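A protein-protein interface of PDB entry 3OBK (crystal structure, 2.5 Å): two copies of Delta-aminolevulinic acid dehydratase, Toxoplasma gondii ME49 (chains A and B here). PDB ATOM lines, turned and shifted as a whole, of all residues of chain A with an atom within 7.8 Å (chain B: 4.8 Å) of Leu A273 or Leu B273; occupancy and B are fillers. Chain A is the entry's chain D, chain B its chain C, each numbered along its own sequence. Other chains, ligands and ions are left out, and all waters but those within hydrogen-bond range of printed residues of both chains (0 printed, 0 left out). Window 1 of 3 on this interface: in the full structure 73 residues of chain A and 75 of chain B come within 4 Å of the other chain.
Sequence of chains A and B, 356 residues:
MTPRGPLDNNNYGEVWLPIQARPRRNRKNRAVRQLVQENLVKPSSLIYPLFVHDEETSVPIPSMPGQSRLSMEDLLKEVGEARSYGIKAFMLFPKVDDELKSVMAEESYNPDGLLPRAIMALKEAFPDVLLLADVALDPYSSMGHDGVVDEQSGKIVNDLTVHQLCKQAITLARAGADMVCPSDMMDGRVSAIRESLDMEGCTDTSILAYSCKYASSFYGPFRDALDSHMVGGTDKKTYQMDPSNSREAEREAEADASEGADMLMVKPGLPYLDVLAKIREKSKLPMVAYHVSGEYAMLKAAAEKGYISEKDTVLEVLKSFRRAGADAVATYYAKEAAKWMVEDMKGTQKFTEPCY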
ATOM      1  N   VAL A 266      18.365 -24.475 -17.626  1.00  0.00           N
ATOM      2  CA  VAL A 266      19.524 -25.151 -17.059  1.00  0.00           C
ATOM      3  C   VAL A 266      19.060 -26.434 -16.379  1.00  0.00           C
ATOM      4  O   VAL A 266      18.090 -26.450 -15.636  1.00  0.00           O
ATOM      5  CB  VAL A 266      20.254 -24.318 -16.000  1.00  0.00           C
ATOM      6  CG1 VAL A 266      21.534 -25.051 -15.551  1.00  0.00           C
ATOM      7  CG2 VAL A 266      20.581 -22.953 -16.520  1.00  0.00           C
ATOM      8  N   PRO A 268      20.837 -30.367 -14.926  1.00  0.00           N
ATOM      9  CA  PRO A 268      20.003 -30.416 -13.724  1.00  0.00           C
ATOM     10  C   PRO A 268      19.967 -29.143 -12.897  1.00  0.00           C
ATOM     11  O   PRO A 268      20.382 -28.060 -13.349  1.00  0.00           O
ATOM     12  CB  PRO A 268      20.645 -31.544 -12.907  1.00  0.00           C
ATOM     13  CG  PRO A 268      21.221 -32.446 -13.915  1.00  0.00           C
ATOM     14  CD  PRO A 268      21.769 -31.510 -14.974  1.00  0.00           C
ATOM     15  N   GLY A 269      19.511 -29.303 -11.662  1.00  0.00           N
ATOM     16  CA  GLY A 269      19.088 -28.167 -10.841  1.00  0.00           C
ATOM     17  C   GLY A 269      20.051 -27.677  -9.788  1.00  0.00           C
ATOM     18  O   GLY A 269      20.909 -26.844 -10.061  1.00  0.00           O
ATOM     19  N   LEU A 270      19.895 -28.180  -8.573  1.00  0.00           N
ATOM     20  CA  LEU A 270      20.735 -27.721  -7.473  1.00  0.00           C
ATOM     21  C   LEU A 270      22.240 -27.816  -7.746  1.00  0.00           C
ATOM     22  O   LEU A 270      22.967 -26.880  -7.494  1.00  0.00           O
ATOM     23  CB  LEU A 270      20.379 -28.436  -6.183  1.00  0.00           C
ATOM     24  CG  LEU A 270      18.995 -28.084  -5.611  1.00  0.00           C
ATOM     25  CD1 LEU A 270      18.839 -28.717  -4.229  1.00  0.00           C
ATOM     26  CD2 LEU A 270      18.766 -26.577  -5.556  1.00  0.00           C
ATOM     27  N   PRO A 271      22.705 -28.923  -8.304  1.00  0.00           N
ATOM     28  CA  PRO A 271      24.136 -29.022  -8.482  1.00  0.00           C
ATOM     29  C   PRO A 271      24.658 -28.225  -9.657  1.00  0.00           C
ATOM     30  O   PRO A 271      25.821 -28.396 -10.029  1.00  0.00           O
ATOM     31  CB  PRO A 271      24.362 -30.517  -8.723  1.00  0.00           C
ATOM     32  CG  PRO A 271      23.104 -31.182  -8.461  1.00  0.00           C
ATOM     33  CD  PRO A 271      22.041 -30.158  -8.713  1.00  0.00           C
ATOM     34  N   TYR A 272      23.820 -27.347 -10.218  1.00  0.00           N
ATOM     35  CA  TYR A 272      24.210 -26.490 -11.314  1.00  0.00           C
ATOM     36  C   TYR A 272      23.818 -25.031 -11.078  1.00  0.00           C
ATOM     37  O   TYR A 272      23.800 -24.202 -12.010  1.00  0.00           O
ATOM     38  CB  TYR A 272      23.634 -27.067 -12.608  1.00  0.00           C
ATOM     39  CG  TYR A 272      24.313 -28.388 -12.955  1.00  0.00           C
ATOM     40  CD1 TYR A 272      25.451 -28.418 -13.745  1.00  0.00           C
ATOM     41  CD2 TYR A 272      23.877 -29.585 -12.404  1.00  0.00           C
ATOM     42  CE1 TYR A 272      26.121 -29.608 -14.009  1.00  0.00           C
ATOM     43  CE2 TYR A 272      24.539 -30.802 -12.684  1.00  0.00           C
ATOM     44  CZ  TYR A 272      25.655 -30.806 -13.485  1.00  0.00           C
ATOM     45  OH  TYR A 272      26.314 -31.978 -13.769  1.00  0.00           O
ATOM     46  N   LEU A 273      23.550 -24.669  -9.831  1.00  0.00           N
ATOM     47  CA  LEU A 273      23.024 -23.320  -9.569  1.00  0.00           C
ATOM     48  C   LEU A 273      24.029 -22.235  -9.991  1.00  0.00           C
ATOM     49  O   LEU A 273      23.607 -21.141 -10.339  1.00  0.00           O
ATOM     50  CB  LEU A 273      22.636 -23.133  -8.098  1.00  0.00           C
ATOM     51  CG  LEU A 273      21.517 -23.963  -7.444  1.00  0.00           C
ATOM     52  CD1 LEU A 273      21.399 -23.572  -5.960  1.00  0.00           C
ATOM     53  CD2 LEU A 273      20.178 -23.859  -8.167  1.00  0.00           C
ATOM     54  N   ASP A 274      25.341 -22.535  -9.940  1.00  0.00           N
ATOM     55  CA  ASP A 274      26.368 -21.625 -10.450  1.00  0.00           C
ATOM     56  C   ASP A 274      26.160 -21.300 -11.941  1.00  0.00           C
ATOM     57  O   ASP A 274      26.346 -20.146 -12.374  1.00  0.00           O
ATOM     58  CB  ASP A 274      27.780 -22.202 -10.257  1.00  0.00           C
ATOM     59  CG  ASP A 274      27.976 -23.524 -10.984  1.00  0.00           C
ATOM     60  OD1 ASP A 274      27.151 -24.425 -10.741  1.00  0.00           O
ATOM     61  OD2 ASP A 274      28.921 -23.663 -11.791  1.00  0.00           O
ATOM     62  N   VAL A 275      25.800 -22.313 -12.725  1.00  0.00           N
ATOM     63  CA  VAL A 275      25.613 -22.112 -14.161  1.00  0.00           C
ATOM     64  C   VAL A 275      24.372 -21.275 -14.396  1.00  0.00           C
ATOM     65  O   VAL A 275      24.369 -20.368 -15.209  1.00  0.00           O
ATOM     66  CB  VAL A 275      25.524 -23.454 -14.954  1.00  0.00           C
ATOM     67  CG1 VAL A 275      25.214 -23.191 -16.427  1.00  0.00           C
ATOM     68  CG2 VAL A 275      26.817 -24.212 -14.818  1.00  0.00           C
ATOM     69  N   LEU A 276      23.328 -21.592 -13.650  1.00  0.00           N
ATOM     70  CA  LEU A 276      22.059 -20.853 -13.641  1.00  0.00           C
ATOM     71  C   LEU A 276      22.262 -19.354 -13.378  1.00  0.00           C
ATOM     72  O   LEU A 276      21.828 -18.516 -14.162  1.00  0.00           O
ATOM     73  CB  LEU A 276      21.124 -21.515 -12.635  1.00  0.00           C
ATOM     74  CG  LEU A 276      19.744 -20.899 -12.415  1.00  0.00           C
ATOM     75  CD1 LEU A 276      18.941 -20.795 -13.720  1.00  0.00           C
ATOM     76  CD2 LEU A 276      18.995 -21.651 -11.328  1.00  0.00           C
ATOM     77  N   ALA A 277      22.970 -19.021 -12.307  1.00  0.00           N
ATOM     78  CA  ALA A 277      23.285 -17.617 -11.980  1.00  0.00           C
ATOM     79  C   ALA A 277      24.061 -16.896 -13.081  1.00  0.00           C
ATOM     80  O   ALA A 277      23.766 -15.749 -13.396  1.00  0.00           O
ATOM     81  CB  ALA A 277      24.073 -17.530 -10.670  1.00  0.00           C
ATOM     82  N   LYS A 278      25.067 -17.558 -13.648  1.00  0.00           N
ATOM     83  CA  LYS A 278      25.919 -16.915 -14.631  1.00  0.00           C
ATOM     84  C   LYS A 278      25.041 -16.629 -15.847  1.00  0.00           C
ATOM     85  O   LYS A 278      25.066 -15.543 -16.393  1.00  0.00           O
ATOM     86  CB  LYS A 278      27.161 -17.770 -15.003  1.00  0.00           C
ATOM     87  N   ILE A 279      24.253 -17.605 -16.264  1.00  0.00           N
ATOM     88  CA  ILE A 279      23.450 -17.399 -17.450  1.00  0.00           C
ATOM     89  C   ILE A 279      22.417 -16.311 -17.205  1.00  0.00           C
ATOM     90  O   ILE A 279      22.193 -15.466 -18.082  1.00  0.00           O
ATOM     91  CB  ILE A 279      22.813 -18.692 -17.979  1.00  0.00           C
ATOM     92  CG1 ILE A 279      23.907 -19.672 -18.430  1.00  0.00           C
ATOM     93  CG2 ILE A 279      21.887 -18.380 -19.147  1.00  0.00           C
ATOM     94  CD1 ILE A 279      24.827 -19.141 -19.553  1.00  0.00           C
ATOM     95  N   ARG A 280      21.826 -16.304 -16.015  1.00  0.00           N
ATOM     96  CA  ARG A 280      20.913 -15.238 -15.606  1.00  0.00           C
ATOM     97  C   ARG A 280      21.521 -13.863 -15.785  1.00  0.00           C
ATOM     98  O   ARG A 280      20.878 -12.964 -16.294  1.00  0.00           O
ATOM     99  CB  ARG A 280      20.535 -15.422 -14.134  1.00  0.00           C
ATOM    100  CG  ARG A 280      19.628 -14.339 -13.555  1.00  0.00           C
ATOM    101  CD  ARG A 280      18.439 -14.227 -14.397  1.00  0.00           C
ATOM    102  NE  ARG A 280      17.286 -13.687 -13.706  1.00  0.00           N
ATOM    103  CZ  ARG A 280      16.898 -12.418 -13.781  1.00  0.00           C
ATOM    104  NH1 ARG A 280      17.597 -11.518 -14.484  1.00  0.00           N
ATOM    105  NH2 ARG A 280      15.783 -12.046 -13.149  1.00  0.00           N
ATOM    106  N   ALA A 289      14.890 -23.524 -14.412  1.00  0.00           N
ATOM    107  CA  ALA A 289      15.768 -24.585 -13.903  1.00  0.00           C
ATOM    108  C   ALA A 289      14.962 -25.853 -13.788  1.00  0.00           C
ATOM    109  O   ALA A 289      13.756 -25.814 -13.560  1.00  0.00           O
ATOM    110  CB  ALA A 289      16.350 -24.207 -12.542  1.00  0.00           C
ATOM    111  N   GLU A 295      17.124 -35.706  -8.203  1.00  0.00           N
ATOM    112  CA  GLU A 295      17.133 -34.736  -7.099  1.00  0.00           C
ATOM    113  C   GLU A 295      15.909 -34.968  -6.241  1.00  0.00           C
ATOM    114  O   GLU A 295      15.980 -34.949  -5.028  1.00  0.00           O
ATOM    115  CB  GLU A 295      17.200 -33.280  -7.623  1.00  0.00           C
ATOM    116  CG  GLU A 295      18.397 -33.001  -8.509  1.00  0.00           C
ATOM    117  CD  GLU A 295      18.457 -31.558  -8.993  1.00  0.00           C
ATOM    118  OE1 GLU A 295      18.814 -30.669  -8.168  1.00  0.00           O
ATOM    119  OE2 GLU A 295      18.159 -31.317 -10.204  1.00  0.00           O
ATOM    120  N   VAL A 317      14.788 -25.497  -0.958  1.00  0.00           N
ATOM    121  CA  VAL A 317      15.343 -25.755  -2.286  1.00  0.00           C
ATOM    122  C   VAL A 317      14.743 -24.816  -3.312  1.00  0.00           C
ATOM    123  O   VAL A 317      15.459 -24.204  -4.091  1.00  0.00           O
ATOM    124  CB  VAL A 317      15.092 -27.218  -2.700  1.00  0.00           C
ATOM    125  CG1 VAL A 317      15.356 -27.426  -4.177  1.00  0.00           C
ATOM    126  CG2 VAL A 317      15.968 -28.147  -1.852  1.00  0.00           C
ATOM    127  N   LYS A 319      13.276 -21.912  -2.956  1.00  0.00           N
ATOM    128  CA  LYS A 319      13.722 -20.550  -2.693  1.00  0.00           C
ATOM    129  C   LYS A 319      15.127 -20.366  -3.261  1.00  0.00           C
ATOM    130  O   LYS A 319      15.432 -19.345  -3.868  1.00  0.00           O
ATOM    131  CB  LYS A 319      13.683 -20.245  -1.162  1.00  0.00           C
ATOM    132  CG  LYS A 319      14.123 -18.852  -0.746  1.00  0.00           C
ATOM    133  CD  LYS A 319      13.278 -17.724  -1.364  1.00  0.00           C
ATOM    134  CE  LYS A 319      11.871 -17.637  -0.787  1.00  0.00           C
ATOM    135  NZ  LYS A 319      11.834 -17.380   0.681  1.00  0.00           N
ATOM    136  N   SER A 320      15.980 -21.361  -3.088  1.00  0.00           N
ATOM    137  CA  SER A 320      17.350 -21.308  -3.651  1.00  0.00           C
ATOM    138  C   SER A 320      17.341 -21.197  -5.159  1.00  0.00           C
ATOM    139  O   SER A 320      18.047 -20.364  -5.744  1.00  0.00           O
ATOM    140  CB  SER A 320      18.154 -22.542  -3.260  1.00  0.00           C
ATOM    141  OG  SER A 320      18.611 -22.428  -1.936  1.00  0.00           O
ATOM    142  N   PHE A 321      16.530 -22.022  -5.800  1.00  0.00           N
ATOM    143  CA  PHE A 321      16.425 -21.957  -7.232  1.00  0.00           C
ATOM    144  C   PHE A 321      16.157 -20.512  -7.650  1.00  0.00           C
ATOM    145  O   PHE A 321      16.807 -19.959  -8.519  1.00  0.00           O
ATOM    146  CB  PHE A 321      15.315 -22.873  -7.727  1.00  0.00           C
ATOM    147  CG  PHE A 321      15.771 -24.238  -8.041  1.00  0.00           C
ATOM    148  CD1 PHE A 321      16.688 -24.446  -9.062  1.00  0.00           C
ATOM    149  CD2 PHE A 321      15.309 -25.323  -7.330  1.00  0.00           C
ATOM    150  CE1 PHE A 321      17.120 -25.722  -9.381  1.00  0.00           C
ATOM    151  CE2 PHE A 321      15.742 -26.594  -7.636  1.00  0.00           C
ATOM    152  CZ  PHE A 321      16.630 -26.788  -8.676  1.00  0.00           C
ATOM    153  N   ARG A 322      15.230 -19.894  -6.966  1.00  0.00           N
ATOM    154  CA  ARG A 322      14.780 -18.555  -7.289  1.00  0.00           C
ATOM    155  C   ARG A 322      15.830 -17.481  -6.988  1.00  0.00           C
ATOM    156  O   ARG A 322      15.992 -16.534  -7.737  1.00  0.00           O
ATOM    157  CB  ARG A 322      13.530 -18.309  -6.471  1.00  0.00           C
ATOM    158  CG  ARG A 322      12.728 -17.147  -6.915  1.00  0.00           C
ATOM    159  CD  ARG A 322      11.498 -17.537  -7.685  1.00  0.00           C
ATOM    160  NE  ARG A 322      10.744 -16.292  -7.845  1.00  0.00           N
ATOM    161  CZ  ARG A 322      10.417 -15.746  -9.004  1.00  0.00           C
ATOM    162  NH1 ARG A 322      10.718 -16.343 -10.154  1.00  0.00           N
ATOM    163  NH2 ARG A 322       9.739 -14.605  -9.006  1.00  0.00           N
ATOM    164  N   ARG A 323      16.556 -17.649  -5.880  1.00  0.00           N
ATOM    165  CA  ARG A 323      17.679 -16.755  -5.566  1.00  0.00           C
ATOM    166  C   ARG A 323      18.782 -16.919  -6.608  1.00  0.00           C
ATOM    167  O   ARG A 323      19.426 -15.960  -6.980  1.00  0.00           O
ATOM    168  CB  ARG A 323      18.250 -17.066  -4.184  1.00  0.00           C
ATOM    169  CG  ARG A 323      19.471 -16.210  -3.777  1.00  0.00           C
ATOM    170  CD  ARG A 323      20.287 -16.845  -2.656  1.00  0.00           C
ATOM    171  NE  ARG A 323      20.819 -18.137  -3.066  1.00  0.00           N
ATOM    172  CZ  ARG A 323      20.467 -19.323  -2.568  1.00  0.00           C
ATOM    173  NH1 ARG A 323      19.567 -19.446  -1.587  1.00  0.00           N
ATOM    174  NH2 ARG A 323      21.038 -20.428  -3.060  1.00  0.00           N
ATOM    175  N   ALA A 324      18.999 -18.157  -7.064  1.00  0.00           N
ATOM    176  CA  ALA A 324      20.063 -18.415  -8.016  1.00  0.00           C
ATOM    177  C   ALA A 324      19.704 -17.792  -9.352  1.00  0.00           C
ATOM    178  O   ALA A 324      20.588 -17.542 -10.149  1.00  0.00           O
ATOM    179  CB  ALA A 324      20.315 -19.895  -8.161  1.00  0.00           C
ATOM    180  N   GLY A 325      18.421 -17.529  -9.596  1.00  0.00           N
ATOM    181  CA  GLY A 325      17.994 -16.842 -10.816  1.00  0.00           C
ATOM    182  C   GLY A 325      17.007 -17.586 -11.690  1.00  0.00           C
ATOM    183  O   GLY A 325      16.861 -17.267 -12.860  1.00  0.00           O
ATOM    184  N   ALA A 326      16.350 -18.607 -11.148  1.00  0.00           N
ATOM    185  CA  ALA A 326      15.294 -19.306 -11.872  1.00  0.00           C
ATOM    186  C   ALA A 326      14.068 -18.414 -11.856  1.00  0.00           C
ATOM    187  O   ALA A 326      13.639 -18.015 -10.794  1.00  0.00           O
ATOM    188  CB  ALA A 326      14.987 -20.625 -11.217  1.00  0.00           C
ATOM    189  N   GLY B 269      25.995 -26.460   0.864  1.00  0.00           N
ATOM    190  CA  GLY B 269      26.735 -26.652  -0.354  1.00  0.00           C
ATOM    191  C   GLY B 269      25.955 -26.424  -1.629  1.00  0.00           C
ATOM    192  O   GLY B 269      25.840 -25.274  -2.101  1.00  0.00           O
ATOM    193  N   LEU B 270      25.425 -27.523  -2.181  1.00  0.00           N
ATOM    194  CA  LEU B 270      24.856 -27.493  -3.524  1.00  0.00           C
ATOM    195  C   LEU B 270      23.713 -26.510  -3.663  1.00  0.00           C
ATOM    196  O   LEU B 270      23.584 -25.894  -4.701  1.00  0.00           O
ATOM    197  CB  LEU B 270      24.360 -28.873  -3.965  1.00  0.00           C
ATOM    198  CG  LEU B 270      25.394 -29.971  -4.097  1.00  0.00           C
ATOM    199  CD1 LEU B 270      24.706 -31.282  -4.465  1.00  0.00           C
ATOM    200  CD2 LEU B 270      26.435 -29.569  -5.117  1.00  0.00           C
ATOM    201  N   PRO B 271      22.860 -26.370  -2.637  1.00  0.00           N
ATOM    202  CA  PRO B 271      21.772 -25.418  -2.788  1.00  0.00           C
ATOM    203  C   PRO B 271      22.219 -23.971  -2.678  1.00  0.00           C
ATOM    204  O   PRO B 271      21.384 -23.058  -2.716  1.00  0.00           O
ATOM    205  CB  PRO B 271      20.801 -25.777  -1.638  1.00  0.00           C
ATOM    206  CG  PRO B 271      21.272 -27.123  -1.145  1.00  0.00           C
ATOM    207  CD  PRO B 271      22.739 -27.133  -1.388  1.00  0.00           C
ATOM    208  N   TYR B 272      23.523 -23.763  -2.550  1.00  0.00           N
ATOM    209  CA  TYR B 272      24.092 -22.416  -2.503  1.00  0.00           C
ATOM    210  C   TYR B 272      25.248 -22.248  -3.458  1.00  0.00           C
ATOM    211  O   TYR B 272      26.103 -21.382  -3.255  1.00  0.00           O
ATOM    212  CB  TYR B 272      24.484 -22.073  -1.064  1.00  0.00           C
ATOM    213  CG  TYR B 272      23.266 -22.085  -0.171  1.00  0.00           C
ATOM    214  CD1 TYR B 272      22.537 -20.931   0.057  1.00  0.00           C
ATOM    215  CD2 TYR B 272      22.821 -23.259   0.403  1.00  0.00           C
ATOM    216  CE1 TYR B 272      21.385 -20.949   0.854  1.00  0.00           C
ATOM    217  CE2 TYR B 272      21.685 -23.286   1.180  1.00  0.00           C
ATOM    218  CZ  TYR B 272      20.968 -22.141   1.401  1.00  0.00           C
ATOM    219  OH  TYR B 272      19.837 -22.191   2.180  1.00  0.00           O
ATOM    220  N   LEU B 273      25.258 -23.031  -4.535  1.00  0.00           N
ATOM    221  CA  LEU B 273      26.320 -22.873  -5.532  1.00  0.00           C
ATOM    222  C   LEU B 273      26.315 -21.475  -6.113  1.00  0.00           C
ATOM    223  O   LEU B 273      27.379 -20.932  -6.391  1.00  0.00           O
ATOM    224  CB  LEU B 273      26.230 -23.904  -6.661  1.00  0.00           C
ATOM    225  CG  LEU B 273      26.525 -25.359  -6.300  1.00  0.00           C
ATOM    226  CD1 LEU B 273      26.653 -26.263  -7.555  1.00  0.00           C
ATOM    227  CD2 LEU B 273      27.757 -25.427  -5.418  1.00  0.00           C
ATOM    228  N   ASP B 274      25.147 -20.857  -6.260  1.00  0.00           N
ATOM    229  CA  ASP B 274      25.119 -19.511  -6.833  1.00  0.00           C
ATOM    230  C   ASP B 274      25.884 -18.537  -5.968  1.00  0.00           C
ATOM    231  O   ASP B 274      26.459 -17.573  -6.470  1.00  0.00           O
ATOM    232  CB  ASP B 274      23.716 -18.992  -7.020  1.00  0.00           C
ATOM    233  CG  ASP B 274      22.901 -19.000  -5.730  1.00  0.00           C
ATOM    234  OD1 ASP B 274      22.781 -20.067  -5.094  1.00  0.00           O
ATOM    235  OD2 ASP B 274      22.368 -17.933  -5.367  1.00  0.00           O
ATOM    236  N   VAL B 275      25.897 -18.795  -4.664  1.00  0.00           N
ATOM    237  CA  VAL B 275      26.501 -17.856  -3.746  1.00  0.00           C
ATOM    238  C   VAL B 275      27.981 -18.116  -3.810  1.00  0.00           C
ATOM    239  O   VAL B 275      28.778 -17.189  -3.884  1.00  0.00           O
ATOM    240  CB  VAL B 275      25.946 -18.014  -2.334  1.00  0.00           C
ATOM    241  CG1 VAL B 275      26.704 -17.123  -1.355  1.00  0.00           C
ATOM    242  CG2 VAL B 275      24.422 -17.709  -2.345  1.00  0.00           C
ATOM    243  N   LEU B 276      28.332 -19.400  -3.831  1.00  0.00           N
ATOM    244  CA  LEU B 276      29.702 -19.808  -3.915  1.00  0.00           C
ATOM    245  C   LEU B 276      30.350 -19.162  -5.120  1.00  0.00           C
ATOM    246  O   LEU B 276      31.389 -18.549  -4.990  1.00  0.00           O
ATOM    247  CB  LEU B 276      29.790 -21.339  -3.983  1.00  0.00           C
ATOM    248  CG  LEU B 276      31.168 -21.979  -4.187  1.00  0.00           C
ATOM    249  CD1 LEU B 276      32.125 -21.630  -3.041  1.00  0.00           C
ATOM    250  CD2 LEU B 276      30.996 -23.476  -4.343  1.00  0.00           C
ATOM    251  N   ALA B 277      29.736 -19.287  -6.294  1.00  0.00           N
ATOM    252  CA  ALA B 277      30.321 -18.686  -7.516  1.00  0.00           C
ATOM    253  C   ALA B 277      30.415 -17.152  -7.419  1.00  0.00           C
ATOM    254  O   ALA B 277      31.371 -16.541  -7.890  1.00  0.00           O
ATOM    255  CB  ALA B 277      29.521 -19.088  -8.738  1.00  0.00           C
ATOM    256  N   SER B 320      30.921 -30.578  -9.446  1.00  0.00           N
ATOM    257  CA  SER B 320      30.069 -29.358  -9.415  1.00  0.00           C
ATOM    258  C   SER B 320      30.561 -28.317  -8.398  1.00  0.00           C
ATOM    259  O   SER B 320      30.643 -27.172  -8.737  1.00  0.00           O
ATOM    260  CB  SER B 320      28.606 -29.699  -9.176  1.00  0.00           C
ATOM    261  OG  SER B 320      28.041 -30.293 -10.341  1.00  0.00           O
ATOM    262  N   PHE B 321      30.912 -28.709  -7.175  1.00  0.00           N
ATOM    263  CA  PHE B 321      31.409 -27.757  -6.176  1.00  0.00           C
ATOM    264  C   PHE B 321      32.627 -27.052  -6.716  1.00  0.00           C
ATOM    265  O   PHE B 321      32.849 -25.864  -6.531  1.00  0.00           O
ATOM    266  CB  PHE B 321      31.877 -28.482  -4.915  1.00  0.00           C
ATOM    267  CG  PHE B 321      30.801 -28.773  -3.937  1.00  0.00           C
ATOM    268  CD1 PHE B 321      30.165 -27.739  -3.292  1.00  0.00           C
ATOM    269  CD2 PHE B 321      30.469 -30.088  -3.619  1.00  0.00           C
ATOM    270  CE1 PHE B 321      29.165 -28.015  -2.379  1.00  0.00           C
ATOM    271  CE2 PHE B 321      29.501 -30.366  -2.719  1.00  0.00           C
ATOM    272  CZ  PHE B 321      28.828 -29.339  -2.093  1.00  0.00           C
ATOM    273  N   ARG B 323      33.620 -26.824  -9.968  1.00  0.00           N
ATOM    274  CA  ARG B 323      33.252 -25.936 -11.069  1.00  0.00           C
ATOM    275  C   ARG B 323      32.625 -24.624 -10.558  1.00  0.00           C
ATOM    276  O   ARG B 323      32.933 -23.556 -11.066  1.00  0.00           O
ATOM    277  CB  ARG B 323      32.310 -26.628 -12.043  1.00  0.00           C
ATOM    278  CG  ARG B 323      31.940 -25.794 -13.257  1.00  0.00           C
ATOM    279  CD  ARG B 323      30.661 -26.291 -13.891  1.00  0.00           C
ATOM    280  NE  ARG B 323      29.537 -26.158 -12.951  1.00  0.00           N
ATOM    281  CZ  ARG B 323      28.901 -27.159 -12.349  1.00  0.00           C
ATOM    282  NH1 ARG B 323      29.199 -28.403 -12.611  1.00  0.00           N
ATOM    283  NH2 ARG B 323      27.920 -26.905 -11.500  1.00  0.00           N
ATOM    284  N   ALA B 324      31.791 -24.707  -9.528  1.00  0.00           N
ATOM    285  CA  ALA B 324      31.126 -23.514  -9.007  1.00  0.00           C
ATOM    286  C   ALA B 324      32.072 -22.544  -8.279  1.00  0.00           C
ATOM    287  O   ALA B 324      31.684 -21.429  -7.967  1.00  0.00           O
ATOM    288  CB  ALA B 324      30.006 -23.910  -8.111  1.00  0.00           C
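The guanidinium group (NH2) of Arg A323 lies within salt-bridge range of the side-chain carboxylate (OD1) of Asp B274, 2.7 Å away. The side-chain hydroxyl of Ser B320 sits at hydrogen-bond distance from the backbone carbonyl oxygen of Pro A271 (2.9 Å). The guanidinium group (NH2) of Arg B323 lies within hydrogen-bond range of the backbone carbonyl oxygen (O) of Pro A271 (3.0 Å). The backbone carbonyl oxygen (O) of Pro B271 lies within hydrogen-bond range of the side-chain hydroxyl (OG) of Ser A320 (2.9 Å). The backbone carbonyl oxygen of Leu B270 lies close to the backbone carbonyl oxygen of Leu A270 (3.0 Å). The guanidinium group (NH2) of Arg B323 is in salt-bridge range of the side-chain carboxylate (OD1) of Asp A274. The guanidinium group of Arg A323 sits at hydrogen-bond distance from the backbone carbonyl oxygen of Pro B271, 2.7 Å away.
Leu B273 touches Pro A271. Leu A273 touches Pro B271. Leu A273 touches Asp B274. Asp A274 touches Leu B273 (N to CB, 3.7 Å). Asp A274 touches Ala B277. CB of Asp A274 touches CB of Ala B324 (3.5 Å). Arg B323 touches Val A275. CB of Ala A277 touches CB of Asp B274, at 3.9 Å. Val B275 touches Arg A323. Asp B274 touches Ala A324.
Printed residues of chain B within 4 Å of Leu A273: Leu B270 (3.4 Å), Pro B271 (3.3 Å), Leu B273 (3.9 Å) and Asp B274 (3.9 Å). Of chain A, only Leu A270, Pro A271, Leu A273 and Asp A274 come within 4 Å of Leu B273. Printed residues of chain B within 4 Å of Ala A277: Asp B274. Of the printed residues of chain A, Ser B320 touches Pro A271 (2.9 Å) and Tyr A272 (3.98 Å). Of the printed residues of chain B, Pro A271 touches Leu B273, Ser B320 and Arg B323. Printed residues of chain B within 4 Å of Leu A270: Leu B270 (3.0 Å) and Leu B273 (3.7 Å). Of the printed residues of chain B, Tyr A272 touches Ser B320 (3.98 Å) and Arg B323 (3.6 Å). Lys A319 touches none of the printed residues of chain B. The nearest residue of chain A that does not touch Leu B273 is Tyr A272 (4.04 Å).
Pro A271 touches Arg B323, and with the chains exchanged Arg A323 touches Pro B271. Tyr A272 touches Ser B320, but with the chains exchanged Ser A320 does not touch Tyr B272 (4.1 Å). Asp A274 touches Ala B277, and with the chains exchanged Ala A277 touches Asp B274. Asp A274 touches Ala B324, and with the chains exchanged Ala A324 touches Asp B274. Of the 23 pairs that touch across the chains among the printed residues, 22 have their exchanged pair printed and touching as well.
Of the 25 printed residues of chain A, 10 touch a printed residue of chain B. Printed residues of chain A that touch a printed residue of chain B: Leu A270, Pro A271, Tyr A272, Leu A273, Asp A274, Val A275, Ala A277, Ser A320, Arg A323 and Ala A324. Hydrophobic or aromatic side chains of chain B within 4 Å of the printed part of chain A: Tyr B272, Leu B273, Val B275, Ala B277 and Ala B324. Among the printed residues, 23 pairs touch across the chains. Among the printed residues, Asp or Glu carboxylates within 4 Å of a Lys or Arg side-chain nitrogen of the other chain: Asp A274 with Arg B323 (2.7 Å) and Arg A323 with Asp B274 (2.7 Å).
The backbone NH (N) of Ala B277 lies close to the backbone carbonyl oxygen (O) of Ala B324 (3.3 Å). The backbone NH (N) of Leu A270 is in hydrogen-bond range of the side-chain carboxylate (OE1) of Glu A295, 2.7 Å away. NH1 of Arg A323 is in hydrogen-bond range of OG of Ser A320 (3.2 Å). The guanidinium group (NH1) of Arg B323 lies within hydrogen-bond range of the side-chain hydroxyl (OG) of Ser B320 (3.2 Å).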
